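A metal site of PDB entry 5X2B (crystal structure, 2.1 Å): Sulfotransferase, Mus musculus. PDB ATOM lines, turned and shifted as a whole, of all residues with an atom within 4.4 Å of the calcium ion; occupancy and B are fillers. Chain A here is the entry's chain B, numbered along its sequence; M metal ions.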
ATOM      1  N   TYR A 124      21.066  12.780  15.782  1.00  0.00           N
ATOM      2  CA  TYR A 124      21.089  12.365  17.178  1.00  0.00           C
ATOM      3  C   TYR A 124      22.493  11.952  17.579  1.00  0.00           C
ATOM      4  O   TYR A 124      22.904  12.079  18.747  1.00  0.00           O
ATOM      5  CB  TYR A 124      20.212  11.140  17.321  1.00  0.00           C
ATOM      6  CG  TYR A 124      18.818  11.352  17.855  1.00  0.00           C
ATOM      7  CD1 TYR A 124      17.853  12.061  17.136  1.00  0.00           C
ATOM      8  CD2 TYR A 124      18.437  10.791  19.042  1.00  0.00           C
ATOM      9  CE1 TYR A 124      16.582  12.224  17.626  1.00  0.00           C
ATOM     10  CE2 TYR A 124      17.169  10.929  19.533  1.00  0.00           C
ATOM     11  CZ  TYR A 124      16.243  11.628  18.836  1.00  0.00           C
ATOM     12  OH  TYR A 124      15.010  11.732  19.403  1.00  0.00           O
ATOM     13  N   ARG A 125      23.171  11.395  16.589  1.00  0.00           N
ATOM     14  CA  ARG A 125      24.520  10.901  16.709  1.00  0.00           C
ATOM     15  C   ARG A 125      25.424  12.105  16.738  1.00  0.00           C
ATOM     16  O   ARG A 125      26.425  12.122  17.437  1.00  0.00           O
ATOM     17  CB  ARG A 125      24.824   9.997  15.498  1.00  0.00           C
ATOM     18  CG  ARG A 125      26.138   9.193  15.518  1.00  0.00           C
ATOM     19  CD  ARG A 125      26.114   8.170  14.384  1.00  0.00           C
ATOM     20  NE  ARG A 125      27.426   7.842  13.866  1.00  0.00           N
ATOM     21  CZ  ARG A 125      27.939   6.606  13.826  1.00  0.00           C
ATOM     22  NH1 ARG A 125      27.258   5.553  14.288  1.00  0.00           N
ATOM     23  NH2 ARG A 125      29.141   6.411  13.328  1.00  0.00           N
ATOM     24  N   ASP A 126      25.061  13.152  16.012  1.00  0.00           N
ATOM     25  CA  ASP A 126      25.939  14.318  15.907  1.00  0.00           C
ATOM     26  C   ASP A 126      25.429  15.566  16.613  1.00  0.00           C
ATOM     27  O   ASP A 126      26.144  16.562  16.686  1.00  0.00           O
ATOM     28  CB  ASP A 126      26.196  14.625  14.437  1.00  0.00           C
ATOM     29  CG  ASP A 126      26.890  13.480  13.735  1.00  0.00           C
ATOM     30  OD1 ASP A 126      27.330  12.564  14.453  1.00  0.00           O
ATOM     31  OD2 ASP A 126      26.997  13.497  12.486  1.00  0.00           O
ATOM     32  N   ASN A 127      24.212  15.523  17.150  1.00  0.00           N
ATOM     33  CA  ASN A 127      23.700  16.672  17.855  1.00  0.00           C
ATOM     34  C   ASN A 127      23.694  16.418  19.332  1.00  0.00           C
ATOM     35  O   ASN A 127      22.836  15.732  19.871  1.00  0.00           O
ATOM     36  CB  ASN A 127      22.312  17.091  17.373  1.00  0.00           C
ATOM     37  CG  ASN A 127      21.891  18.431  17.902  1.00  0.00           C
ATOM     38  OD1 ASN A 127      22.409  18.900  18.918  1.00  0.00           O
ATOM     39  ND2 ASN A 127      20.962  19.060  17.216  1.00  0.00           N
ATOM     40  N   PRO A 128      24.646  17.012  20.003  1.00  0.00           N
ATOM     41  CA  PRO A 128      24.697  16.916  21.458  1.00  0.00           C
ATOM     42  C   PRO A 128      23.429  17.382  22.016  1.00  0.00           C
ATOM     43  O   PRO A 128      23.138  17.076  23.163  1.00  0.00           O
ATOM     44  CB  PRO A 128      25.833  17.853  21.822  1.00  0.00           C
ATOM     45  CG  PRO A 128      25.913  18.846  20.651  1.00  0.00           C
ATOM     46  CD  PRO A 128      25.594  18.001  19.467  1.00  0.00           C
ATOM     47  N   LEU A 130      20.907  16.153  21.186  1.00  0.00           N
ATOM     48  CA  LEU A 130      20.088  14.990  21.122  1.00  0.00           C
ATOM     49  C   LEU A 130      20.886  13.844  21.610  1.00  0.00           C
ATOM     50  O   LEU A 130      22.114  13.865  21.537  1.00  0.00           O
ATOM     51  CB  LEU A 130      19.730  14.726  19.709  1.00  0.00           C
ATOM     52  CG  LEU A 130      19.106  15.946  19.085  1.00  0.00           C
ATOM     53  CD1 LEU A 130      18.981  15.751  17.621  1.00  0.00           C
ATOM     54  CD2 LEU A 130      17.794  16.119  19.714  1.00  0.00           C
ATOM     55  N   PRO A 131      20.179  12.835  22.105  1.00  0.00           N
ATOM     56  CA  PRO A 131      20.734  11.676  22.808  1.00  0.00           C
ATOM     57  C   PRO A 131      21.104  10.571  21.885  1.00  0.00           C
ATOM     58  O   PRO A 131      20.262   9.777  21.525  1.00  0.00           O
ATOM     59  CB  PRO A 131      19.562  11.226  23.675  1.00  0.00           C
ATOM     60  CG  PRO A 131      18.392  11.623  22.919  1.00  0.00           C
ATOM     61  CD  PRO A 131      18.730  12.933  22.271  1.00  0.00           C
ATOM     62  N   SER A 132      22.359  10.511  21.518  1.00  0.00           N
ATOM     63  CA  SER A 132      22.854   9.441  20.694  1.00  0.00           C
ATOM     64  C   SER A 132      22.206   8.045  20.953  1.00  0.00           C
ATOM     65  O   SER A 132      22.012   7.655  22.095  1.00  0.00           O
ATOM     66  CB  SER A 132      24.367   9.343  20.908  1.00  0.00           C
ATOM     67  OG  SER A 132      24.836   8.048  20.515  1.00  0.00           O
HETATM   68 CA    CA M   1      23.844  13.909  20.265  1.00  0.00          CA
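The backbone carbonyl oxygen of Tyr 124 lies close to the backbone NH of Ser 132 (3.2 Å).
Residues that only touch the calcium ion: Pro 128 (3.2 Å) and Ser 132 (3.9 Å).
Within 4 Å of the calcium ion: Tyr 124, Asn 127, Pro 128, Leu 130 and Ser 132.
The nearest printed residue that does not touch the calcium ion is Arg 125 (4.2 Å).
The calcium ion is bound by the backbone carbonyl oxygen (O) of Asn 127 (2.1 Å), the backbone carbonyl oxygen (O) of Leu 130 (2.1 Å) and the backbone carbonyl oxygen (O) of Tyr 124 (2.6 Å).
The calcium ion has three donor atoms within binding distance.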
